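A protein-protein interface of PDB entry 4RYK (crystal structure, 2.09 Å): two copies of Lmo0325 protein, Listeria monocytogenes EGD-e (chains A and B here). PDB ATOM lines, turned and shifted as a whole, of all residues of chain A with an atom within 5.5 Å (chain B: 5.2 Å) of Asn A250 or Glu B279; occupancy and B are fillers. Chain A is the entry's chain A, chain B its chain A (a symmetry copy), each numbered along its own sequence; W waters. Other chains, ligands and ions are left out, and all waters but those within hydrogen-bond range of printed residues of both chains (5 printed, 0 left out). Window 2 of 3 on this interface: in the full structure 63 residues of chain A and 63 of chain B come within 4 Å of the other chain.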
ATOM      1  N   LYS A 231      -1.594  33.027 -24.344  1.00  0.00           N
ATOM      2  CA  LYS A 231      -0.648  32.822 -25.446  1.00  0.00           C
ATOM      3  C   LYS A 231       0.637  33.594 -25.196  1.00  0.00           C
ATOM      4  O   LYS A 231       1.734  33.015 -25.208  1.00  0.00           O
ATOM      5  CB  LYS A 231      -1.208  33.277 -26.779  1.00  0.00           C
ATOM      6  CG  LYS A 231      -2.312  32.411 -27.347  1.00  0.00           C
ATOM      7  CD  LYS A 231      -1.748  31.186 -28.036  1.00  0.00           C
ATOM      8  CE  LYS A 231      -2.801  30.373 -28.801  1.00  0.00           C
ATOM      9  NZ  LYS A 231      -2.115  29.318 -29.617  1.00  0.00           N
ATOM     10  N   TYR A 245       1.588  25.002 -21.012  1.00  0.00           N
ATOM     11  CA  TYR A 245       0.543  25.973 -21.186  1.00  0.00           C
ATOM     12  C   TYR A 245       0.345  26.418 -22.621  1.00  0.00           C
ATOM     13  O   TYR A 245      -0.693  26.966 -22.958  1.00  0.00           O
ATOM     14  CB  TYR A 245       0.755  27.172 -20.253  1.00  0.00           C
ATOM     15  CG  TYR A 245       0.453  26.790 -18.840  1.00  0.00           C
ATOM     16  CD1 TYR A 245      -0.837  26.595 -18.432  1.00  0.00           C
ATOM     17  CD2 TYR A 245       1.468  26.573 -17.935  1.00  0.00           C
ATOM     18  CE1 TYR A 245      -1.151  26.193 -17.131  1.00  0.00           C
ATOM     19  CE2 TYR A 245       1.190  26.176 -16.645  1.00  0.00           C
ATOM     20  CZ  TYR A 245      -0.133  26.008 -16.241  1.00  0.00           C
ATOM     21  OH  TYR A 245      -0.405  25.652 -14.942  1.00  0.00           O
ATOM     22  N   ARG A 246       1.314  26.171 -23.494  1.00  0.00           N
ATOM     23  CA  ARG A 246       1.103  26.393 -24.919  1.00  0.00           C
ATOM     24  C   ARG A 246       0.113  25.350 -25.437  1.00  0.00           C
ATOM     25  O   ARG A 246      -0.642  25.602 -26.366  1.00  0.00           O
ATOM     26  CB  ARG A 246       2.421  26.331 -25.682  1.00  0.00           C
ATOM     27  CG  ARG A 246       3.393  27.389 -25.205  1.00  0.00           C
ATOM     28  CD  ARG A 246       4.562  27.468 -26.148  1.00  0.00           C
ATOM     29  NE  ARG A 246       5.623  28.346 -25.674  1.00  0.00           N
ATOM     30  CZ  ARG A 246       6.650  28.730 -26.415  1.00  0.00           C
ATOM     31  NH1 ARG A 246       6.741  28.307 -27.651  1.00  0.00           N
ATOM     32  NH2 ARG A 246       7.593  29.520 -25.922  1.00  0.00           N
ATOM     33  N   ILE A 247       0.088  24.169 -24.817  1.00  0.00           N
ATOM     34  CA  ILE A 247      -0.842  23.138 -25.244  1.00  0.00           C
ATOM     35  C   ILE A 247      -2.241  23.592 -24.819  1.00  0.00           C
ATOM     36  O   ILE A 247      -3.213  23.537 -25.596  1.00  0.00           O
ATOM     37  CB  ILE A 247      -0.538  21.757 -24.625  1.00  0.00           C
ATOM     38  CG1 ILE A 247       0.876  21.273 -24.950  1.00  0.00           C
ATOM     39  CG2 ILE A 247      -1.521  20.714 -25.155  1.00  0.00           C
ATOM     40  CD1 ILE A 247       1.285  20.097 -24.061  1.00  0.00           C
ATOM     41  N   VAL A 248      -2.311  24.059 -23.587  1.00  0.00           N
ATOM     42  CA  VAL A 248      -3.569  24.586 -23.029  1.00  0.00           C
ATOM     43  C   VAL A 248      -4.123  25.682 -23.913  1.00  0.00           C
ATOM     44  O   VAL A 248      -5.324  25.650 -24.276  1.00  0.00           O
ATOM     45  CB  VAL A 248      -3.393  25.099 -21.609  1.00  0.00           C
ATOM     46  CG1 VAL A 248      -4.718  25.656 -21.098  1.00  0.00           C
ATOM     47  CG2 VAL A 248      -2.909  23.998 -20.673  1.00  0.00           C
ATOM     48  N   ALA A 249      -3.259  26.634 -24.280  1.00  0.00           N
ATOM     49  CA  ALA A 249      -3.653  27.722 -25.210  1.00  0.00           C
ATOM     50  C   ALA A 249      -4.150  27.195 -26.562  1.00  0.00           C
ATOM     51  O   ALA A 249      -5.140  27.694 -27.105  1.00  0.00           O
ATOM     52  CB  ALA A 249      -2.501  28.683 -25.428  1.00  0.00           C
ATOM     53  N   ASN A 250      -3.491  26.163 -27.090  1.00  0.00           N
ATOM     54  CA  ASN A 250      -3.957  25.556 -28.330  1.00  0.00           C
ATOM     55  C   ASN A 250      -5.341  24.942 -28.166  1.00  0.00           C
ATOM     56  O   ASN A 250      -6.178  25.087 -29.069  1.00  0.00           O
ATOM     57  CB  ASN A 250      -3.007  24.483 -28.879  1.00  0.00           C
ATOM     58  CG  ASN A 250      -1.757  25.064 -29.554  1.00  0.00           C
ATOM     59  OD1 ASN A 250      -1.683  26.250 -29.873  1.00  0.00           O
ATOM     60  ND2 ASN A 250      -0.775  24.202 -29.794  1.00  0.00           N
ATOM     61  N   TYR A 251      -5.575  24.247 -27.039  1.00  0.00           N
ATOM     62  CA  TYR A 251      -6.886  23.716 -26.741  1.00  0.00           C
ATOM     63  C   TYR A 251      -7.976  24.823 -26.752  1.00  0.00           C
ATOM     64  O   TYR A 251      -8.986  24.724 -27.445  1.00  0.00           O
ATOM     65  CB  TYR A 251      -6.918  22.978 -25.394  1.00  0.00           C
ATOM     66  CG  TYR A 251      -8.326  22.518 -25.127  1.00  0.00           C
ATOM     67  CD1 TYR A 251      -9.226  23.336 -24.466  1.00  0.00           C
ATOM     68  CD2 TYR A 251      -8.770  21.285 -25.599  1.00  0.00           C
ATOM     69  CE1 TYR A 251     -10.553  22.945 -24.276  1.00  0.00           C
ATOM     70  CE2 TYR A 251     -10.069  20.875 -25.426  1.00  0.00           C
ATOM     71  CZ  TYR A 251     -10.974  21.706 -24.770  1.00  0.00           C
ATOM     72  OH  TYR A 251     -12.270  21.266 -24.612  1.00  0.00           O
ATOM     73  N   TYR A 252      -7.778  25.867 -25.970  1.00  0.00           N
ATOM     74  CA  TYR A 252      -8.789  26.935 -25.905  1.00  0.00           C
ATOM     75  C   TYR A 252      -8.992  27.727 -27.217  1.00  0.00           C
ATOM     76  O   TYR A 252     -10.106  28.168 -27.501  1.00  0.00           O
ATOM     77  CB  TYR A 252      -8.542  27.862 -24.694  1.00  0.00           C
ATOM     78  CG  TYR A 252      -8.842  27.170 -23.381  1.00  0.00           C
ATOM     79  CD1 TYR A 252     -10.130  26.724 -23.085  1.00  0.00           C
ATOM     80  CD2 TYR A 252      -7.862  26.971 -22.433  1.00  0.00           C
ATOM     81  CE1 TYR A 252     -10.418  26.090 -21.888  1.00  0.00           C
ATOM     82  CE2 TYR A 252      -8.134  26.321 -21.225  1.00  0.00           C
ATOM     83  CZ  TYR A 252      -9.396  25.864 -20.971  1.00  0.00           C
ATOM     84  OH  TYR A 252      -9.676  25.227 -19.789  1.00  0.00           O
ATOM     85  N   GLN A 253      -7.955  27.859 -28.035  1.00  0.00           N
ATOM     86  CA  GLN A 253      -8.064  28.534 -29.334  1.00  0.00           C
ATOM     87  C   GLN A 253      -8.986  27.669 -30.204  1.00  0.00           C
ATOM     88  O   GLN A 253      -9.855  28.175 -30.946  1.00  0.00           O
ATOM     89  CB  GLN A 253      -6.692  28.724 -29.979  1.00  0.00           C
ATOM     90  CG  GLN A 253      -6.702  29.386 -31.353  1.00  0.00           C
ATOM     91  CD  GLN A 253      -7.380  30.757 -31.341  1.00  0.00           C
ATOM     92  OE1 GLN A 253      -6.711  31.753 -31.161  1.00  0.00           O
ATOM     93  NE2 GLN A 253      -8.716  30.800 -31.466  1.00  0.00           N
ATOM     94  N   GLY A 254      -8.851  26.353 -30.035  1.00  0.00           N
ATOM     95  CA  GLY A 254      -9.710  25.409 -30.727  1.00  0.00           C
ATOM     96  C   GLY A 254     -11.165  25.610 -30.362  1.00  0.00           C
ATOM     97  O   GLY A 254     -12.017  25.719 -31.223  1.00  0.00           O
ATOM     98  N   ALA A 255     -11.432  25.687 -29.070  1.00  0.00           N
ATOM     99  CA  ALA A 255     -12.795  25.841 -28.580  1.00  0.00           C
ATOM    100  C   ALA A 255     -13.411  27.153 -29.080  1.00  0.00           C
ATOM    101  O   ALA A 255     -14.555  27.185 -29.515  1.00  0.00           O
ATOM    102  CB  ALA A 255     -12.786  25.818 -27.054  1.00  0.00           C
ATOM    103  N   GLN A 269      -8.064  21.181 -33.808  1.00  0.00           N
ATOM    104  CA  GLN A 269      -7.040  21.754 -32.984  1.00  0.00           C
ATOM    105  C   GLN A 269      -7.177  21.283 -31.544  1.00  0.00           C
ATOM    106  O   GLN A 269      -6.187  20.994 -30.896  1.00  0.00           O
ATOM    107  CB  GLN A 269      -7.148  23.248 -33.037  1.00  0.00           C
ATOM    108  CG  GLN A 269      -6.306  23.951 -31.997  1.00  0.00           C
ATOM    109  CD  GLN A 269      -5.223  24.751 -32.606  1.00  0.00           C
ATOM    110  OE1 GLN A 269      -4.791  24.460 -33.706  1.00  0.00           O
ATOM    111  NE2 GLN A 269      -4.808  25.794 -31.918  1.00  0.00           N
ATOM    112  N   ALA A 270      -8.403  21.251 -31.042  1.00  0.00           N
ATOM    113  CA  ALA A 270      -8.683  20.799 -29.677  1.00  0.00           C
ATOM    114  C   ALA A 270      -8.327  19.325 -29.490  1.00  0.00           C
ATOM    115  O   ALA A 270      -7.742  18.950 -28.483  1.00  0.00           O
ATOM    116  CB  ALA A 270     -10.156  21.020 -29.343  1.00  0.00           C
ATOM    117  N   ARG A 272      -6.122  17.775 -31.248  1.00  0.00           N
ATOM    118  CA  ARG A 272      -4.681  17.687 -31.343  1.00  0.00           C
ATOM    119  C   ARG A 272      -4.021  18.024 -29.971  1.00  0.00           C
ATOM    120  O   ARG A 272      -3.037  17.396 -29.560  1.00  0.00           O
ATOM    121  CB  ARG A 272      -4.203  18.596 -32.444  1.00  0.00           C
ATOM    122  CG  ARG A 272      -2.716  18.751 -32.484  1.00  0.00           C
ATOM    123  CD  ARG A 272      -2.142  17.716 -33.383  1.00  0.00           C
ATOM    124  NE  ARG A 272      -1.988  16.382 -32.823  1.00  0.00           N
ATOM    125  CZ  ARG A 272      -0.927  15.941 -32.136  1.00  0.00           C
ATOM    126  NH1 ARG A 272      -0.896  14.671 -31.741  1.00  0.00           N
ATOM    127  NH2 ARG A 272       0.096  16.745 -31.834  1.00  0.00           N
ATOM    128  N   ALA A 273      -4.573  18.989 -29.243  1.00  0.00           N
ATOM    129  CA  ALA A 273      -4.027  19.306 -27.948  1.00  0.00           C
ATOM    130  C   ALA A 273      -4.167  18.108 -26.983  1.00  0.00           C
ATOM    131  O   ALA A 273      -3.221  17.755 -26.287  1.00  0.00           O
ATOM    132  CB  ALA A 273      -4.687  20.530 -27.375  1.00  0.00           C
ATOM    133  N   THR A 276      -1.711  15.528 -27.792  1.00  0.00           N
ATOM    134  CA  THR A 276      -0.400  15.982 -27.422  1.00  0.00           C
ATOM    135  C   THR A 276      -0.175  15.741 -25.957  1.00  0.00           C
ATOM    136  O   THR A 276       0.887  15.270 -25.566  1.00  0.00           O
ATOM    137  CB  THR A 276      -0.172  17.457 -27.769  1.00  0.00           C
ATOM    138  OG1 THR A 276      -0.229  17.630 -29.191  1.00  0.00           O
ATOM    139  CG2 THR A 276       1.202  17.872 -27.319  1.00  0.00           C
ATOM    140  N   ARG B 272       7.133  13.023 -35.081  1.00  0.00           N
ATOM    141  CA  ARG B 272       6.051  13.530 -34.267  1.00  0.00           C
ATOM    142  C   ARG B 272       6.581  14.584 -33.247  1.00  0.00           C
ATOM    143  O   ARG B 272       5.933  15.605 -32.983  1.00  0.00           O
ATOM    144  CB  ARG B 272       5.363  12.376 -33.587  1.00  0.00           C
ATOM    145  CG  ARG B 272       4.373  12.801 -32.550  1.00  0.00           C
ATOM    146  CD  ARG B 272       3.035  12.944 -33.184  1.00  0.00           C
ATOM    147  NE  ARG B 272       2.794  14.176 -33.919  1.00  0.00           N
ATOM    148  CZ  ARG B 272       2.334  15.320 -33.399  1.00  0.00           C
ATOM    149  NH1 ARG B 272       2.097  16.349 -34.207  1.00  0.00           N
ATOM    150  NH2 ARG B 272       2.114  15.454 -32.088  1.00  0.00           N
ATOM    151  N   GLN B 275       7.086  17.849 -35.197  1.00  0.00           N
ATOM    152  CA  GLN B 275       5.780  18.456 -35.457  1.00  0.00           C
ATOM    153  C   GLN B 275       5.189  19.076 -34.209  1.00  0.00           C
ATOM    154  O   GLN B 275       4.495  20.080 -34.281  1.00  0.00           O
ATOM    155  CB  GLN B 275       4.840  17.381 -36.004  1.00  0.00           C
ATOM    156  CG  GLN B 275       3.442  17.807 -36.426  1.00  0.00           C
ATOM    157  CD  GLN B 275       3.375  18.942 -37.441  1.00  0.00           C
ATOM    158  OE1 GLN B 275       4.236  19.077 -38.335  1.00  0.00           O
ATOM    159  NE2 GLN B 275       2.316  19.780 -37.307  1.00  0.00           N
ATOM    160  N   THR B 276       5.449  18.457 -33.060  1.00  0.00           N
ATOM    161  CA  THR B 276       4.945  18.947 -31.809  1.00  0.00           C
ATOM    162  C   THR B 276       5.622  20.243 -31.461  1.00  0.00           C
ATOM    163  O   THR B 276       4.964  21.186 -31.038  1.00  0.00           O
ATOM    164  CB  THR B 276       5.109  17.931 -30.673  1.00  0.00           C
ATOM    165  OG1 THR B 276       4.319  16.768 -30.953  1.00  0.00           O
ATOM    166  CG2 THR B 276       4.598  18.525 -29.389  1.00  0.00           C
ATOM    167  N   TRP B 277       6.938  20.319 -31.634  1.00  0.00           N
ATOM    168  CA  TRP B 277       7.600  21.597 -31.414  1.00  0.00           C
ATOM    169  C   TRP B 277       7.000  22.692 -32.329  1.00  0.00           C
ATOM    170  O   TRP B 277       6.854  23.859 -31.904  1.00  0.00           O
ATOM    171  CB  TRP B 277       9.105  21.514 -31.649  1.00  0.00           C
ATOM    172  CG  TRP B 277       9.870  20.942 -30.487  1.00  0.00           C
ATOM    173  CD1 TRP B 277       9.813  21.352 -29.203  1.00  0.00           C
ATOM    174  CD2 TRP B 277      10.825  19.900 -30.533  1.00  0.00           C
ATOM    175  NE1 TRP B 277      10.655  20.628 -28.436  1.00  0.00           N
ATOM    176  CE2 TRP B 277      11.278  19.704 -29.233  1.00  0.00           C
ATOM    177  CE3 TRP B 277      11.300  19.064 -31.545  1.00  0.00           C
ATOM    178  CZ2 TRP B 277      12.227  18.748 -28.912  1.00  0.00           C
ATOM    179  CZ3 TRP B 277      12.207  18.100 -31.227  1.00  0.00           C
ATOM    180  CH2 TRP B 277      12.676  17.958 -29.915  1.00  0.00           C
ATOM    181  N   LYS B 278       6.651  22.329 -33.560  1.00  0.00           N
ATOM    182  CA  LYS B 278       6.032  23.301 -34.467  1.00  0.00           C
ATOM    183  C   LYS B 278       4.692  23.733 -33.972  1.00  0.00           C
ATOM    184  O   LYS B 278       4.409  24.921 -33.973  1.00  0.00           O
ATOM    185  CB  LYS B 278       5.844  22.784 -35.880  1.00  0.00           C
ATOM    186  CG  LYS B 278       7.161  22.693 -36.597  1.00  0.00           C
ATOM    187  CD  LYS B 278       7.015  22.121 -37.987  1.00  0.00           C
ATOM    188  CE  LYS B 278       8.386  21.892 -38.585  1.00  0.00           C
ATOM    189  NZ  LYS B 278       8.278  21.292 -39.938  1.00  0.00           N
ATOM    190  N   GLU B 279       3.894  22.771 -33.540  1.00  0.00           N
ATOM    191  CA  GLU B 279       2.525  23.073 -33.134  1.00  0.00           C
ATOM    192  C   GLU B 279       2.484  23.932 -31.883  1.00  0.00           C
ATOM    193  O   GLU B 279       1.518  24.649 -31.661  1.00  0.00           O
ATOM    194  CB  GLU B 279       1.793  21.793 -32.893  1.00  0.00           C
ATOM    195  CG  GLU B 279       1.517  21.051 -34.173  1.00  0.00           C
ATOM    196  CD  GLU B 279       0.912  19.692 -33.914  1.00  0.00           C
ATOM    197  OE1 GLU B 279       0.914  19.271 -32.740  1.00  0.00           O
ATOM    198  OE2 GLU B 279       0.436  19.058 -34.865  1.00  0.00           O
ATOM    199  N   LEU B 280       3.549  23.842 -31.080  1.00  0.00           N
ATOM    200  CA  LEU B 280       3.660  24.612 -29.851  1.00  0.00           C
ATOM    201  C   LEU B 280       4.516  25.862 -30.018  1.00  0.00           C
ATOM    202  O   LEU B 280       4.885  26.456 -29.026  1.00  0.00           O
ATOM    203  CB  LEU B 280       4.202  23.774 -28.670  1.00  0.00           C
ATOM    204  CG  LEU B 280       3.413  22.502 -28.322  1.00  0.00           C
ATOM    205  CD1 LEU B 280       4.071  21.777 -27.171  1.00  0.00           C
ATOM    206  CD2 LEU B 280       1.980  22.806 -27.939  1.00  0.00           C
ATOM    207  N   HIS B 281       4.767  26.269 -31.253  1.00  0.00           N
ATOM    208  CA  HIS B 281       5.356  27.573 -31.592  1.00  0.00           C
ATOM    209  C   HIS B 281       6.839  27.642 -31.128  1.00  0.00           C
ATOM    210  O   HIS B 281       7.335  28.695 -30.739  1.00  0.00           O
ATOM    211  CB  HIS B 281       4.467  28.721 -31.071  1.00  0.00           C
ATOM    212  CG  HIS B 281       2.996  28.428 -31.167  1.00  0.00           C
ATOM    213  ND1 HIS B 281       2.326  28.360 -32.365  1.00  0.00           N
ATOM    214  CD2 HIS B 281       2.074  28.147 -30.212  1.00  0.00           C
ATOM    215  CE1 HIS B 281       1.069  28.026 -32.153  1.00  0.00           C
ATOM    216  NE2 HIS B 281       0.889  27.894 -30.853  1.00  0.00           N
HETATM  217  O   HOH W   1       0.434  31.247 -30.706  1.00  0.00           O
HETATM  218  O   HOH W   2       0.658  19.942 -30.226  1.00  0.00           O
HETATM  219  O   HOH W   3       9.276  29.861 -28.210  1.00  0.00           O
HETATM  220  O   HOH W   4      -0.172  27.890 -27.868  1.00  0.00           O
HETATM  221  O   HOH W   5      -0.663  24.671 -33.109  1.00  0.00           O
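The side-chain carboxylate (OE1) of Glu B279 lies within salt-bridge range of the guanidinium group (NH2) of Arg A272 (2.8 Å). The guanidinium group (NH2) of Arg B272 sits close to the guanidinium group (NH2) of Arg A272 (2.4 Å). OD1 of Asn A250 is in hydrogen-bond range of NE2 of His B281 (3.2 Å). The side-chain amide nitrogen (ND2) of Asn A250 lies within hydrogen-bond range of the backbone carbonyl oxygen (O) of Glu B279 (3.0 Å). The guanidinium group (NH1) of Arg A246 lies within hydrogen-bond range of the backbone carbonyl oxygen (O) of Leu B280 (3.0 Å). The backbone carbonyl oxygen (O) of His B281 is in hydrogen-bond range of the guanidinium group (NH1) of Arg A246, 3.2 Å away.
NH2 of Arg A272 sits at hydrogen-bond distance from OG1 of Thr A276, at 2.8 Å. The backbone carbonyl oxygen of Asn A250 lies close to the side-chain amide nitrogen of Gln A269 (3.2 Å). NE2 of Gln B275 sits at hydrogen-bond distance from OE2 of Glu B279 (3.2 Å). The guanidinium group (NH1) of Arg B272 lies within salt-bridge range of the side-chain carboxylate (OE2) of Glu B279 (3.2 Å). A ring nitrogen (NE2) of His B281 is in hydrogen-bond range of the backbone carbonyl oxygen of Glu B279 (3.4 Å). The guanidinium group (NH2) of Arg B272 is in hydrogen-bond range of the side-chain hydroxyl (OG1) of Thr B276, 2.8 Å away.
His B281 touches Lys A231 (NE2 to NZ, 3.5 Å). Leu B280 touches Ile A247. Leu B280 touches Asn A250 (CD2 to ND2, 3.6 Å).
Of the printed residues of chain B, Lys A231 touches His B281 (3.5 Å). Asn A250 touches three residues of chain B. Ala A273 touches none of the printed residues of chain B. Glu B279 touches two residues of chain A. Of the printed residues of chain A, Leu B280 touches Arg A246 (3.0 Å), Ile A247 (3.5 Å) and Asn A250 (3.6 Å). The nearest printed residue of chain A that does not touch Arg B272 is Thr A276 (4.3 Å).
Printed residues of chain A that touch a printed residue of chain B: Lys A231, Arg A246, Ile A247, Asn A250 and Arg A272. Printed residues of chain B that touch a printed residue of chain A: Arg B272, Glu B279, Leu B280 and His B281. Among the printed residues, 9 pairs touch across the chains. Among the printed residues, Asp or Glu carboxylates within 4 Å of a Lys or Arg side-chain nitrogen of the other chain: Arg A272 with Glu B279 (2.8 Å).
Arg B272 touches its own counterpart, Arg A272. Positions printed for both chains: 272 and 276. Of the 9 pairs that touch across the chains among the printed residues, 1 has its exchanged pair printed and touching as well.
Water W2 bridges OE1 of Glu B279 (2.6 Å) and OG1 of Thr A276 (2.7 Å). Water W5 bridges O of Glu B279 and ND2 of Asn A250. Water W4 lies within hydrogen-bond range of the backbone carbonyl oxygen of Arg A246 (2.8 Å), the side-chain amino group of Lys A231 (3.0 Å), the side-chain amide oxygen of Asn A250 (3.0 Å) and a ring nitrogen (NE2) of His B281 (3.2 Å). Water W3 bridges the guanidinium group of Arg A246 and the backbone carbonyl oxygen of His B281. Water W1 lies within hydrogen-bond range of NZ of Lys A231 (3.4 Å) and NE2 of His B281 (3.4 Å).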
